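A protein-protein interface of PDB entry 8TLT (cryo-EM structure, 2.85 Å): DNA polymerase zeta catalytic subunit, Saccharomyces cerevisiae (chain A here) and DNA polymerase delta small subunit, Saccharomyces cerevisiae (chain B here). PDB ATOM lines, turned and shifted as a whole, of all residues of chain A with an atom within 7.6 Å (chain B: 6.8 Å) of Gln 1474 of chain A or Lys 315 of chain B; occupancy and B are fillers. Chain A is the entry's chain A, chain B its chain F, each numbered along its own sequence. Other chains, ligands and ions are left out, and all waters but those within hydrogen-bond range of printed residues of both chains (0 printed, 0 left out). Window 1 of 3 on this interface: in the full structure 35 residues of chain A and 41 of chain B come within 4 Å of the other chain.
Among the printed residues, merely in contact across the chains: Leu 1463 of chain A with Pro 312 of chain B (3.7 Å), Leu 1467 of chain A with Ile 275 of chain B (3.9 Å), Leu 1467 of chain A with Asp 311 of chain B (3.98 Å), Leu 1467 of chain A with Pro 312 of chain B (3.7 Å), Leu 1467 of chain A with Ser 313 of chain B (3.2 Å), Leu 1467 of chain A with Lys 315 of chain B (3.9 Å), Lys 1468 of chain A with Ile 275 of chain B (3.2 Å), Gln 1470 of chain A with Asp 314 of chain B (3.7 Å), Gln 1474 of chain A with Lys 315 of chain B (3.5 Å), Thr 1475 of chain A with Val 129 of chain B (3.6 Å) and Val 1479 of chain A with Val 129 of chain B (3.7 Å).
O of Lys 1471 of chain A is in hydrogen-bond range of OG1 of Thr 1475 of chain A (2.9 Å).
The side-chain carboxylate of Asp 311 of chain B is in hydrogen-bond range of the backbone NH of Gly 308 of chain B (3.3 Å).
O of Gln 1474 of chain A sits at hydrogen-bond distance from OG1 of Thr 1478 of chain A, 2.9 Å away.
Gln 1474 of chain A touches just one residue of chain B: Lys 315.
Of chain A, only Leu 1467 (3.9 Å), Gln 1470 (3.5 Å) and Gln 1474 (3.5 Å) come within 4 Å of Lys 315 of chain B.
Of the printed residues of chain B, Leu 1463 of chain A touches Pro 312 (3.7 Å).
Printed residues of chain A within 4 Å of Asp 311 of chain B: Leu 1467.
Trp 424 of chain B touches none of the printed residues of chain A.
Lys 1471 of chain A touches none of the printed residues of chain B.
The nearest residue of chain B that does not touch Gln 1474 of chain A is Ser 316 of chain B (5.2 Å).
The nearest printed residue of chain A that does not touch Asp 311 of chain B is Leu 1463 of chain A (7.3 Å).
Of the 19 printed residues of chain A, 7 touch a printed residue of chain B.
Among the printed residues, 12 pairs touch across the chains.
The side-chain amide nitrogen (NE2) of Gln 1470 of chain A lies close to the backbone NH (N) of Lys 315 of chain B, 3.5 Å away.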
ATOM      1  N   LEU A1463       4.501 -22.440   8.047  1.00  0.00           N
ATOM      2  CA  LEU A1463       3.969 -21.291   7.328  1.00  0.00           C
ATOM      3  C   LEU A1463       2.454 -21.226   7.440  1.00  0.00           C
ATOM      4  O   LEU A1463       1.890 -20.144   7.616  1.00  0.00           O
ATOM      5  CB  LEU A1463       4.396 -21.354   5.862  1.00  0.00           C
ATOM      6  CG  LEU A1463       5.744 -20.726   5.512  1.00  0.00           C
ATOM      7  CD1 LEU A1463       5.983 -20.798   4.016  1.00  0.00           C
ATOM      8  CD2 LEU A1463       5.807 -19.289   5.996  1.00  0.00           C
ATOM      9  N   LYS A1466       1.536 -19.984  10.970  1.00  0.00           N
ATOM     10  CA  LYS A1466       1.847 -18.568  11.133  1.00  0.00           C
ATOM     11  C   LYS A1466       0.882 -17.694  10.341  1.00  0.00           C
ATOM     12  O   LYS A1466       0.419 -16.661  10.840  1.00  0.00           O
ATOM     13  CB  LYS A1466       3.289 -18.298  10.706  1.00  0.00           C
ATOM     14  CG  LYS A1466       3.795 -16.918  11.074  1.00  0.00           C
ATOM     15  CD  LYS A1466       5.256 -16.747  10.700  1.00  0.00           C
ATOM     16  CE  LYS A1466       5.516 -17.194   9.274  1.00  0.00           C
ATOM     17  NZ  LYS A1466       6.391 -16.234   8.548  1.00  0.00           N
ATOM     18  N   LEU A1467       0.566 -18.093   9.108  1.00  0.00           N
ATOM     19  CA  LEU A1467      -0.327 -17.298   8.274  1.00  0.00           C
ATOM     20  C   LEU A1467      -1.745 -17.299   8.823  1.00  0.00           C
ATOM     21  O   LEU A1467      -2.437 -16.277   8.758  1.00  0.00           O
ATOM     22  CB  LEU A1467      -0.304 -17.818   6.838  1.00  0.00           C
ATOM     23  CG  LEU A1467       0.989 -17.620   6.045  1.00  0.00           C
ATOM     24  CD1 LEU A1467       0.682 -17.512   4.565  1.00  0.00           C
ATOM     25  CD2 LEU A1467       1.758 -16.403   6.532  1.00  0.00           C
ATOM     26  N   LYS A1468      -2.200 -18.432   9.363  1.00  0.00           N
ATOM     27  CA  LYS A1468      -3.515 -18.467   9.992  1.00  0.00           C
ATOM     28  C   LYS A1468      -3.580 -17.500  11.166  1.00  0.00           C
ATOM     29  O   LYS A1468      -4.539 -16.726  11.303  1.00  0.00           O
ATOM     30  CB  LYS A1468      -3.838 -19.888  10.451  1.00  0.00           C
ATOM     31  CG  LYS A1468      -4.806 -20.624   9.553  1.00  0.00           C
ATOM     32  CD  LYS A1468      -5.182 -21.973  10.135  1.00  0.00           C
ATOM     33  CE  LYS A1468      -6.341 -21.846  11.106  1.00  0.00           C
ATOM     34  NZ  LYS A1468      -7.032 -23.148  11.317  1.00  0.00           N
ATOM     35  N   ARG A1469      -2.550 -17.517  12.017  1.00  0.00           N
ATOM     36  CA  ARG A1469      -2.536 -16.605  13.157  1.00  0.00           C
ATOM     37  C   ARG A1469      -2.507 -15.149  12.703  1.00  0.00           C
ATOM     38  O   ARG A1469      -3.222 -14.303  13.256  1.00  0.00           O
ATOM     39  CB  ARG A1469      -1.349 -16.917  14.064  1.00  0.00           C
ATOM     40  CG  ARG A1469      -1.388 -18.311  14.666  1.00  0.00           C
ATOM     41  CD  ARG A1469      -0.862 -18.322  16.095  1.00  0.00           C
ATOM     42  NE  ARG A1469      -1.225 -19.527  16.836  1.00  0.00           N
ATOM     43  CZ  ARG A1469      -2.464 -19.935  17.079  1.00  0.00           C
ATOM     44  NH1 ARG A1469      -3.517 -19.231  16.696  1.00  0.00           N
ATOM     45  NH2 ARG A1469      -2.654 -21.074  17.737  1.00  0.00           N
ATOM     46  N   GLN A1470      -1.694 -14.840  11.689  1.00  0.00           N
ATOM     47  CA  GLN A1470      -1.606 -13.466  11.202  1.00  0.00           C
ATOM     48  C   GLN A1470      -2.927 -12.996  10.607  1.00  0.00           C
ATOM     49  O   GLN A1470      -3.346 -11.856  10.836  1.00  0.00           O
ATOM     50  CB  GLN A1470      -0.485 -13.340  10.172  1.00  0.00           C
ATOM     51  CG  GLN A1470       0.908 -13.493  10.745  1.00  0.00           C
ATOM     52  CD  GLN A1470       1.986 -13.221   9.720  1.00  0.00           C
ATOM     53  OE1 GLN A1470       2.840 -14.067   9.460  1.00  0.00           O
ATOM     54  NE2 GLN A1470       1.954 -12.033   9.129  1.00  0.00           N
ATOM     55  N   LYS A1471      -3.592 -13.852   9.827  1.00  0.00           N
ATOM     56  CA  LYS A1471      -4.871 -13.471   9.238  1.00  0.00           C
ATOM     57  C   LYS A1471      -5.926 -13.248  10.312  1.00  0.00           C
ATOM     58  O   LYS A1471      -6.715 -12.296  10.230  1.00  0.00           O
ATOM     59  CB  LYS A1471      -5.332 -14.536   8.244  1.00  0.00           C
ATOM     60  N   GLU A1472      -5.958 -14.111  11.331  1.00  0.00           N
ATOM     61  CA  GLU A1472      -6.910 -13.915  12.421  1.00  0.00           C
ATOM     62  C   GLU A1472      -6.648 -12.603  13.151  1.00  0.00           C
ATOM     63  O   GLU A1472      -7.586 -11.858  13.467  1.00  0.00           O
ATOM     64  CB  GLU A1472      -6.848 -15.097  13.387  1.00  0.00           C
ATOM     65  CG  GLU A1472      -7.572 -14.867  14.703  1.00  0.00           C
ATOM     66  N   TYR A1473      -5.376 -12.293  13.416  1.00  0.00           N
ATOM     67  CA  TYR A1473      -5.053 -11.041  14.093  1.00  0.00           C
ATOM     68  C   TYR A1473      -5.431  -9.834  13.242  1.00  0.00           C
ATOM     69  O   TYR A1473      -5.920  -8.826  13.765  1.00  0.00           O
ATOM     70  CB  TYR A1473      -3.569 -11.000  14.451  1.00  0.00           C
ATOM     71  CG  TYR A1473      -3.203  -9.834  15.338  1.00  0.00           C
ATOM     72  CD1 TYR A1473      -4.016  -9.465  16.400  1.00  0.00           C
ATOM     73  CD2 TYR A1473      -2.051  -9.097  15.108  1.00  0.00           C
ATOM     74  CE1 TYR A1473      -3.690  -8.400  17.211  1.00  0.00           C
ATOM     75  CE2 TYR A1473      -1.716  -8.029  15.915  1.00  0.00           C
ATOM     76  CZ  TYR A1473      -2.539  -7.684  16.965  1.00  0.00           C
ATOM     77  OH  TYR A1473      -2.210  -6.620  17.771  1.00  0.00           O
ATOM     78  N   GLN A1474      -5.202  -9.912  11.929  1.00  0.00           N
ATOM     79  CA  GLN A1474      -5.571  -8.807  11.049  1.00  0.00           C
ATOM     80  C   GLN A1474      -7.079  -8.598  11.026  1.00  0.00           C
ATOM     81  O   GLN A1474      -7.557  -7.457  11.037  1.00  0.00           O
ATOM     82  CB  GLN A1474      -5.042  -9.060   9.638  1.00  0.00           C
ATOM     83  CG  GLN A1474      -3.591  -8.671   9.441  1.00  0.00           C
ATOM     84  CD  GLN A1474      -3.187  -8.665   7.981  1.00  0.00           C
ATOM     85  N   THR A1475      -7.848  -9.689  10.989  1.00  0.00           N
ATOM     86  CA  THR A1475      -9.302  -9.565  11.037  1.00  0.00           C
ATOM     87  C   THR A1475      -9.756  -8.932  12.346  1.00  0.00           C
ATOM     88  O   THR A1475     -10.637  -8.061  12.355  1.00  0.00           O
ATOM     89  CB  THR A1475      -9.955 -10.933  10.848  1.00  0.00           C
ATOM     90  OG1 THR A1475      -9.491 -11.522   9.628  1.00  0.00           O
ATOM     91  CG2 THR A1475     -11.464 -10.799  10.794  1.00  0.00           C
ATOM     92  N   LEU A1476      -9.160  -9.351  13.466  1.00  0.00           N
ATOM     93  CA  LEU A1476      -9.518  -8.765  14.755  1.00  0.00           C
ATOM     94  C   LEU A1476      -9.193  -7.277  14.796  1.00  0.00           C
ATOM     95  O   LEU A1476      -9.982  -6.475  15.311  1.00  0.00           O
ATOM     96  CB  LEU A1476      -8.799  -9.501  15.883  1.00  0.00           C
ATOM     97  CG  LEU A1476      -9.351 -10.882  16.226  1.00  0.00           C
ATOM     98  CD1 LEU A1476      -8.604 -11.471  17.404  1.00  0.00           C
ATOM     99  CD2 LEU A1476     -10.837 -10.801  16.520  1.00  0.00           C
ATOM    100  N   LYS A1477      -8.032  -6.890  14.266  1.00  0.00           N
ATOM    101  CA  LYS A1477      -7.659  -5.480  14.254  1.00  0.00           C
ATOM    102  C   LYS A1477      -8.603  -4.665  13.379  1.00  0.00           C
ATOM    103  O   LYS A1477      -8.957  -3.535  13.731  1.00  0.00           O
ATOM    104  CB  LYS A1477      -6.215  -5.319  13.785  1.00  0.00           C
ATOM    105  CG  LYS A1477      -5.188  -5.607  14.862  1.00  0.00           C
ATOM    106  CD  LYS A1477      -3.776  -5.422  14.340  1.00  0.00           C
ATOM    107  CE  LYS A1477      -3.487  -3.961  14.043  1.00  0.00           C
ATOM    108  NZ  LYS A1477      -2.070  -3.750  13.644  1.00  0.00           N
ATOM    109  N   THR A1478      -9.018  -5.215  12.236  1.00  0.00           N
ATOM    110  CA  THR A1478      -9.983  -4.515  11.394  1.00  0.00           C
ATOM    111  C   THR A1478     -11.314  -4.335  12.115  1.00  0.00           C
ATOM    112  O   THR A1478     -11.930  -3.263  12.044  1.00  0.00           O
ATOM    113  CB  THR A1478     -10.187  -5.271  10.081  1.00  0.00           C
ATOM    114  OG1 THR A1478      -8.926  -5.436   9.423  1.00  0.00           O
ATOM    115  CG2 THR A1478     -11.126  -4.504   9.167  1.00  0.00           C
ATOM    116  N   VAL A1479     -11.769  -5.374  12.817  1.00  0.00           N
ATOM    117  CA  VAL A1479     -13.020  -5.279  13.567  1.00  0.00           C
ATOM    118  C   VAL A1479     -12.917  -4.199  14.637  1.00  0.00           C
ATOM    119  O   VAL A1479     -13.825  -3.375  14.806  1.00  0.00           O
ATOM    120  CB  VAL A1479     -13.382  -6.645  14.178  1.00  0.00           C
ATOM    121  CG1 VAL A1479     -14.411  -6.481  15.281  1.00  0.00           C
ATOM    122  CG2 VAL A1479     -13.895  -7.587  13.106  1.00  0.00           C
ATOM    123  N   CYS A1480     -11.802  -4.184  15.372  1.00  0.00           N
ATOM    124  CA  CYS A1480     -11.629  -3.196  16.433  1.00  0.00           C
ATOM    125  C   CYS A1480     -11.542  -1.781  15.870  1.00  0.00           C
ATOM    126  O   CYS A1480     -12.059  -0.838  16.475  1.00  0.00           O
ATOM    127  CB  CYS A1480     -10.388  -3.526  17.258  1.00  0.00           C
ATOM    128  SG  CYS A1480     -10.646  -4.829  18.477  1.00  0.00           S
ATOM    129  N   ARG A1481     -10.881  -1.612  14.725  1.00  0.00           N
ATOM    130  CA  ARG A1481     -10.799  -0.296  14.097  1.00  0.00           C
ATOM    131  C   ARG A1481     -12.174   0.192  13.657  1.00  0.00           C
ATOM    132  O   ARG A1481     -12.533   1.358  13.877  1.00  0.00           O
ATOM    133  CB  ARG A1481      -9.838  -0.361  12.913  1.00  0.00           C
ATOM    134  CG  ARG A1481      -9.496   0.970  12.287  1.00  0.00           C
ATOM    135  CD  ARG A1481      -8.593   0.766  11.081  1.00  0.00           C
ATOM    136  NE  ARG A1481      -7.546  -0.212  11.353  1.00  0.00           N
ATOM    137  CZ  ARG A1481      -7.337  -1.309  10.637  1.00  0.00           C
ATOM    138  NH1 ARG A1481      -8.082  -1.599   9.585  1.00  0.00           N
ATOM    139  NH2 ARG A1481      -6.355  -2.134  10.987  1.00  0.00           N
ATOM    140  N   ALA A1516      -4.604 -13.566  20.826  1.00  0.00           N
ATOM    141  CA  ALA A1516      -3.847 -13.580  19.579  1.00  0.00           C
ATOM    142  C   ALA A1516      -2.503 -12.883  19.734  1.00  0.00           C
ATOM    143  O   ALA A1516      -1.486 -13.360  19.215  1.00  0.00           O
ATOM    144  CB  ALA A1516      -4.662 -12.932  18.462  1.00  0.00           C
ATOM    145  N   LEU A1520       1.141 -14.613  19.248  1.00  0.00           N
ATOM    146  CA  LEU A1520       2.152 -14.088  18.335  1.00  0.00           C
ATOM    147  C   LEU A1520       3.461 -13.803  19.060  1.00  0.00           C
ATOM    148  O   LEU A1520       4.544 -14.007  18.498  1.00  0.00           O
ATOM    149  CB  LEU A1520       1.635 -12.827  17.642  1.00  0.00           C
ATOM    150  CG  LEU A1520       0.553 -13.012  16.573  1.00  0.00           C
ATOM    151  CD1 LEU A1520       0.537 -11.835  15.612  1.00  0.00           C
ATOM    152  CD2 LEU A1520       0.747 -14.314  15.815  1.00  0.00           C
ATOM    153  N   VAL B 129     -15.301  -9.636   7.537  1.00  0.00           N
ATOM    154  CA  VAL B 129     -14.619  -9.635   8.830  1.00  0.00           C
ATOM    155  C   VAL B 129     -15.554  -9.973   9.985  1.00  0.00           C
ATOM    156  O   VAL B 129     -15.086 -10.448  11.028  1.00  0.00           O
ATOM    157  CB  VAL B 129     -13.925  -8.290   9.106  1.00  0.00           C
ATOM    158  CG1 VAL B 129     -12.911  -7.982   8.018  1.00  0.00           C
ATOM    159  CG2 VAL B 129     -14.943  -7.171   9.230  1.00  0.00           C
ATOM    160  N   ILE B 275      -6.397 -19.775   3.677  1.00  0.00           N
ATOM    161  CA  ILE B 275      -5.591 -20.150   4.835  1.00  0.00           C
ATOM    162  C   ILE B 275      -6.455 -20.729   5.945  1.00  0.00           C
ATOM    163  O   ILE B 275      -5.981 -21.543   6.747  1.00  0.00           O
ATOM    164  CB  ILE B 275      -4.775 -18.945   5.339  1.00  0.00           C
ATOM    165  CG1 ILE B 275      -5.480 -17.635   4.987  1.00  0.00           C
ATOM    166  CG2 ILE B 275      -3.364 -18.982   4.775  1.00  0.00           C
ATOM    167  N   GLY B 308       2.855 -12.864  -3.321  1.00  0.00           N
ATOM    168  CA  GLY B 308       1.542 -12.284  -3.478  1.00  0.00           C
ATOM    169  C   GLY B 308       0.749 -12.310  -2.182  1.00  0.00           C
ATOM    170  O   GLY B 308       1.224 -12.764  -1.138  1.00  0.00           O
ATOM    171  N   THR B 309      -0.485 -11.808  -2.275  1.00  0.00           N
ATOM    172  CA  THR B 309      -1.344 -11.727  -1.097  1.00  0.00           C
ATOM    173  C   THR B 309      -1.739 -13.112  -0.600  1.00  0.00           C
ATOM    174  O   THR B 309      -1.606 -13.415   0.591  1.00  0.00           O
ATOM    175  CB  THR B 309      -2.587 -10.891  -1.411  1.00  0.00           C
ATOM    176  OG1 THR B 309      -2.240  -9.502  -1.413  1.00  0.00           O
ATOM    177  CG2 THR B 309      -3.670 -11.128  -0.373  1.00  0.00           C
ATOM    178  N   ASN B 310      -2.214 -13.973  -1.497  1.00  0.00           N
ATOM    179  CA  ASN B 310      -2.641 -15.313  -1.121  1.00  0.00           C
ATOM    180  C   ASN B 310      -1.523 -16.339  -1.236  1.00  0.00           C
ATOM    181  O   ASN B 310      -1.761 -17.527  -1.001  1.00  0.00           O
ATOM    182  CB  ASN B 310      -3.835 -15.751  -1.974  1.00  0.00           C
ATOM    183  CG  ASN B 310      -3.680 -15.364  -3.422  1.00  0.00           C
ATOM    184  OD1 ASN B 310      -2.572 -15.108  -3.885  1.00  0.00           O
ATOM    185  ND2 ASN B 310      -4.791 -15.311  -4.146  1.00  0.00           N
ATOM    186  N   ASP B 311      -0.320 -15.909  -1.602  1.00  0.00           N
ATOM    187  CA  ASP B 311       0.832 -16.785  -1.591  1.00  0.00           C
ATOM    188  C   ASP B 311       1.226 -17.103  -0.151  1.00  0.00           C
ATOM    189  O   ASP B 311       0.907 -16.347   0.770  1.00  0.00           O
ATOM    190  CB  ASP B 311       1.994 -16.127  -2.329  1.00  0.00           C
ATOM    191  CG  ASP B 311       1.937 -16.361  -3.821  1.00  0.00           C
ATOM    192  OD1 ASP B 311       0.946 -16.957  -4.288  1.00  0.00           O
ATOM    193  OD2 ASP B 311       2.872 -15.938  -4.530  1.00  0.00           O
ATOM    194  N   PRO B 312       1.919 -18.221   0.073  1.00  0.00           N
ATOM    195  CA  PRO B 312       2.350 -18.547   1.439  1.00  0.00           C
ATOM    196  C   PRO B 312       3.429 -17.602   1.947  1.00  0.00           C
ATOM    197  O   PRO B 312       4.606 -17.966   2.021  1.00  0.00           O
ATOM    198  CB  PRO B 312       2.870 -19.985   1.313  1.00  0.00           C
ATOM    199  CG  PRO B 312       3.190 -20.153  -0.128  1.00  0.00           C
ATOM    200  CD  PRO B 312       2.197 -19.318  -0.869  1.00  0.00           C
ATOM    201  N   SER B 313       3.029 -16.383   2.299  1.00  0.00           N
ATOM    202  CA  SER B 313       3.945 -15.385   2.831  1.00  0.00           C
ATOM    203  C   SER B 313       3.175 -14.490   3.792  1.00  0.00           C
ATOM    204  O   SER B 313       1.946 -14.555   3.883  1.00  0.00           O
ATOM    205  CB  SER B 313       4.594 -14.565   1.712  1.00  0.00           C
ATOM    206  N   ASP B 314       3.913 -13.644   4.507  1.00  0.00           N
ATOM    207  CA  ASP B 314       3.313 -12.826   5.553  1.00  0.00           C
ATOM    208  C   ASP B 314       2.304 -11.843   4.971  1.00  0.00           C
ATOM    209  O   ASP B 314       2.431 -11.383   3.834  1.00  0.00           O
ATOM    210  CB  ASP B 314       4.395 -12.077   6.329  1.00  0.00           C
ATOM    211  CG  ASP B 314       5.390 -11.387   5.423  1.00  0.00           C
ATOM    212  OD1 ASP B 314       5.960 -12.066   4.544  1.00  0.00           O
ATOM    213  OD2 ASP B 314       5.607 -10.170   5.594  1.00  0.00           O
ATOM    214  N   LYS B 315       1.284 -11.527   5.773  1.00  0.00           N
ATOM    215  CA  LYS B 315       0.183 -10.692   5.308  1.00  0.00           C
ATOM    216  C   LYS B 315       0.559  -9.220   5.205  1.00  0.00           C
ATOM    217  O   LYS B 315      -0.123  -8.471   4.499  1.00  0.00           O
ATOM    218  CB  LYS B 315      -1.020 -10.859   6.236  1.00  0.00           C
ATOM    219  CG  LYS B 315      -1.431 -12.305   6.450  1.00  0.00           C
ATOM    220  CD  LYS B 315      -1.736 -12.989   5.133  1.00  0.00           C
ATOM    221  CE  LYS B 315      -2.162 -14.429   5.343  1.00  0.00           C
ATOM    222  NZ  LYS B 315      -2.410 -15.124   4.051  1.00  0.00           N
ATOM    223  N   SER B 316       1.611  -8.785   5.891  1.00  0.00           N
ATOM    224  CA  SER B 316       2.058  -7.408   5.768  1.00  0.00           C
ATOM    225  C   SER B 316       2.648  -7.164   4.382  1.00  0.00           C
ATOM    226  O   SER B 316       3.110  -8.085   3.706  1.00  0.00           O
ATOM    227  CB  SER B 316       3.089  -7.081   6.847  1.00  0.00           C
ATOM    228  N   LEU B 317       2.618  -5.899   3.960  1.00  0.00           N
ATOM    229  CA  LEU B 317       3.078  -5.559   2.614  1.00  0.00           C
ATOM    230  C   LEU B 317       4.542  -5.899   2.368  1.00  0.00           C
ATOM    231  O   LEU B 317       4.846  -6.458   1.301  1.00  0.00           O
ATOM    232  CB  LEU B 317       2.801  -4.081   2.324  1.00  0.00           C
ATOM    233  CG  LEU B 317       2.849  -3.712   0.841  1.00  0.00           C
ATOM    234  N   PRO B 318       5.498  -5.593   3.269  1.00  0.00           N
ATOM    235  CA  PRO B 318       6.885  -5.999   2.998  1.00  0.00           C
ATOM    236  C   PRO B 318       7.067  -7.501   3.116  1.00  0.00           C
ATOM    237  O   PRO B 318       7.697  -7.987   4.060  1.00  0.00           O
ATOM    238  CB  PRO B 318       7.690  -5.244   4.062  1.00  0.00           C
ATOM    239  CG  PRO B 318       6.729  -5.016   5.160  1.00  0.00           C
ATOM    240  CD  PRO B 318       5.404  -4.788   4.502  1.00  0.00           C
ATOM    241  N   GLN B 319       6.516  -8.246   2.161  1.00  0.00           N
ATOM    242  CA  GLN B 319       6.593  -9.699   2.202  1.00  0.00           C
ATOM    243  C   GLN B 319       8.009 -10.167   1.901  1.00  0.00           C
ATOM    244  O   GLN B 319       8.644  -9.698   0.951  1.00  0.00           O
ATOM    245  CB  GLN B 319       5.613 -10.314   1.206  1.00  0.00           C
ATOM    246  CG  GLN B 319       4.259  -9.641   1.182  1.00  0.00           C
ATOM    247  CD  GLN B 319       3.169 -10.554   0.675  1.00  0.00           C
ATOM    248  OE1 GLN B 319       3.386 -11.745   0.470  1.00  0.00           O
ATOM    249  NE2 GLN B 319       1.981  -9.999   0.471  1.00  0.00           N
ATOM    250  N   LYS B 365      -0.984  -4.879  -3.355  1.00  0.00           N
ATOM    251  CA  LYS B 365      -1.751  -4.832  -2.115  1.00  0.00           C
ATOM    252  C   LYS B 365      -2.096  -3.402  -1.720  1.00  0.00           C
ATOM    253  O   LYS B 365      -3.148  -3.168  -1.118  1.00  0.00           O
ATOM    254  CB  LYS B 365      -0.991  -5.518  -0.985  1.00  0.00           C
ATOM    255  CG  LYS B 365      -1.864  -5.822   0.221  1.00  0.00           C
ATOM    256  CD  LYS B 365      -1.041  -6.155   1.447  1.00  0.00           C
ATOM    257  CE  LYS B 365      -1.923  -6.685   2.560  1.00  0.00           C
ATOM    258  NZ  LYS B 365      -3.123  -5.835   2.769  1.00  0.00           N
ATOM    259  N   ASP B 421      -3.837  -0.593   7.103  1.00  0.00           N
ATOM    260  CA  ASP B 421      -4.379  -1.701   6.329  1.00  0.00           C
ATOM    261  C   ASP B 421      -3.318  -2.451   5.536  1.00  0.00           C
ATOM    262  O   ASP B 421      -3.492  -3.642   5.258  1.00  0.00           O
ATOM    263  CB  ASP B 421      -5.460  -1.190   5.371  1.00  0.00           C
ATOM    264  CG  ASP B 421      -6.799  -1.863   5.591  1.00  0.00           C
ATOM    265  N   THR B 422      -2.220  -1.787   5.173  1.00  0.00           N
ATOM    266  CA  THR B 422      -1.224  -2.356   4.271  1.00  0.00           C
ATOM    267  C   THR B 422      -0.042  -2.988   4.996  1.00  0.00           C
ATOM    268  O   THR B 422       0.287  -4.148   4.739  1.00  0.00           O
ATOM    269  CB  THR B 422      -0.720  -1.277   3.304  1.00  0.00           C
ATOM    270  OG1 THR B 422      -1.815  -0.453   2.890  1.00  0.00           O
ATOM    271  CG2 THR B 422      -0.091  -1.910   2.082  1.00  0.00           C
ATOM    272  N   LEU B 423       0.606  -2.255   5.896  1.00  0.00           N
ATOM    273  CA  LEU B 423       1.844  -2.704   6.513  1.00  0.00           C
ATOM    274  C   LEU B 423       1.662  -2.932   8.008  1.00  0.00           C
ATOM    275  O   LEU B 423       0.871  -2.253   8.669  1.00  0.00           O
ATOM    276  CB  LEU B 423       2.972  -1.695   6.280  1.00  0.00           C
ATOM    277  CG  LEU B 423       2.599  -0.216   6.364  1.00  0.00           C
ATOM    278  CD2 LEU B 423       3.444   0.600   5.406  1.00  0.00           C
ATOM    279  N   TRP B 424       2.405  -3.904   8.532  1.00  0.00           N
ATOM    280  CA  TRP B 424       2.401  -4.224   9.950  1.00  0.00           C
ATOM    281  C   TRP B 424       3.435  -3.363  10.676  1.00  0.00           C
ATOM    282  O   TRP B 424       3.963  -2.392  10.128  1.00  0.00           O
ATOM    283  CB  TRP B 424       2.662  -5.715  10.159  1.00  0.00           C
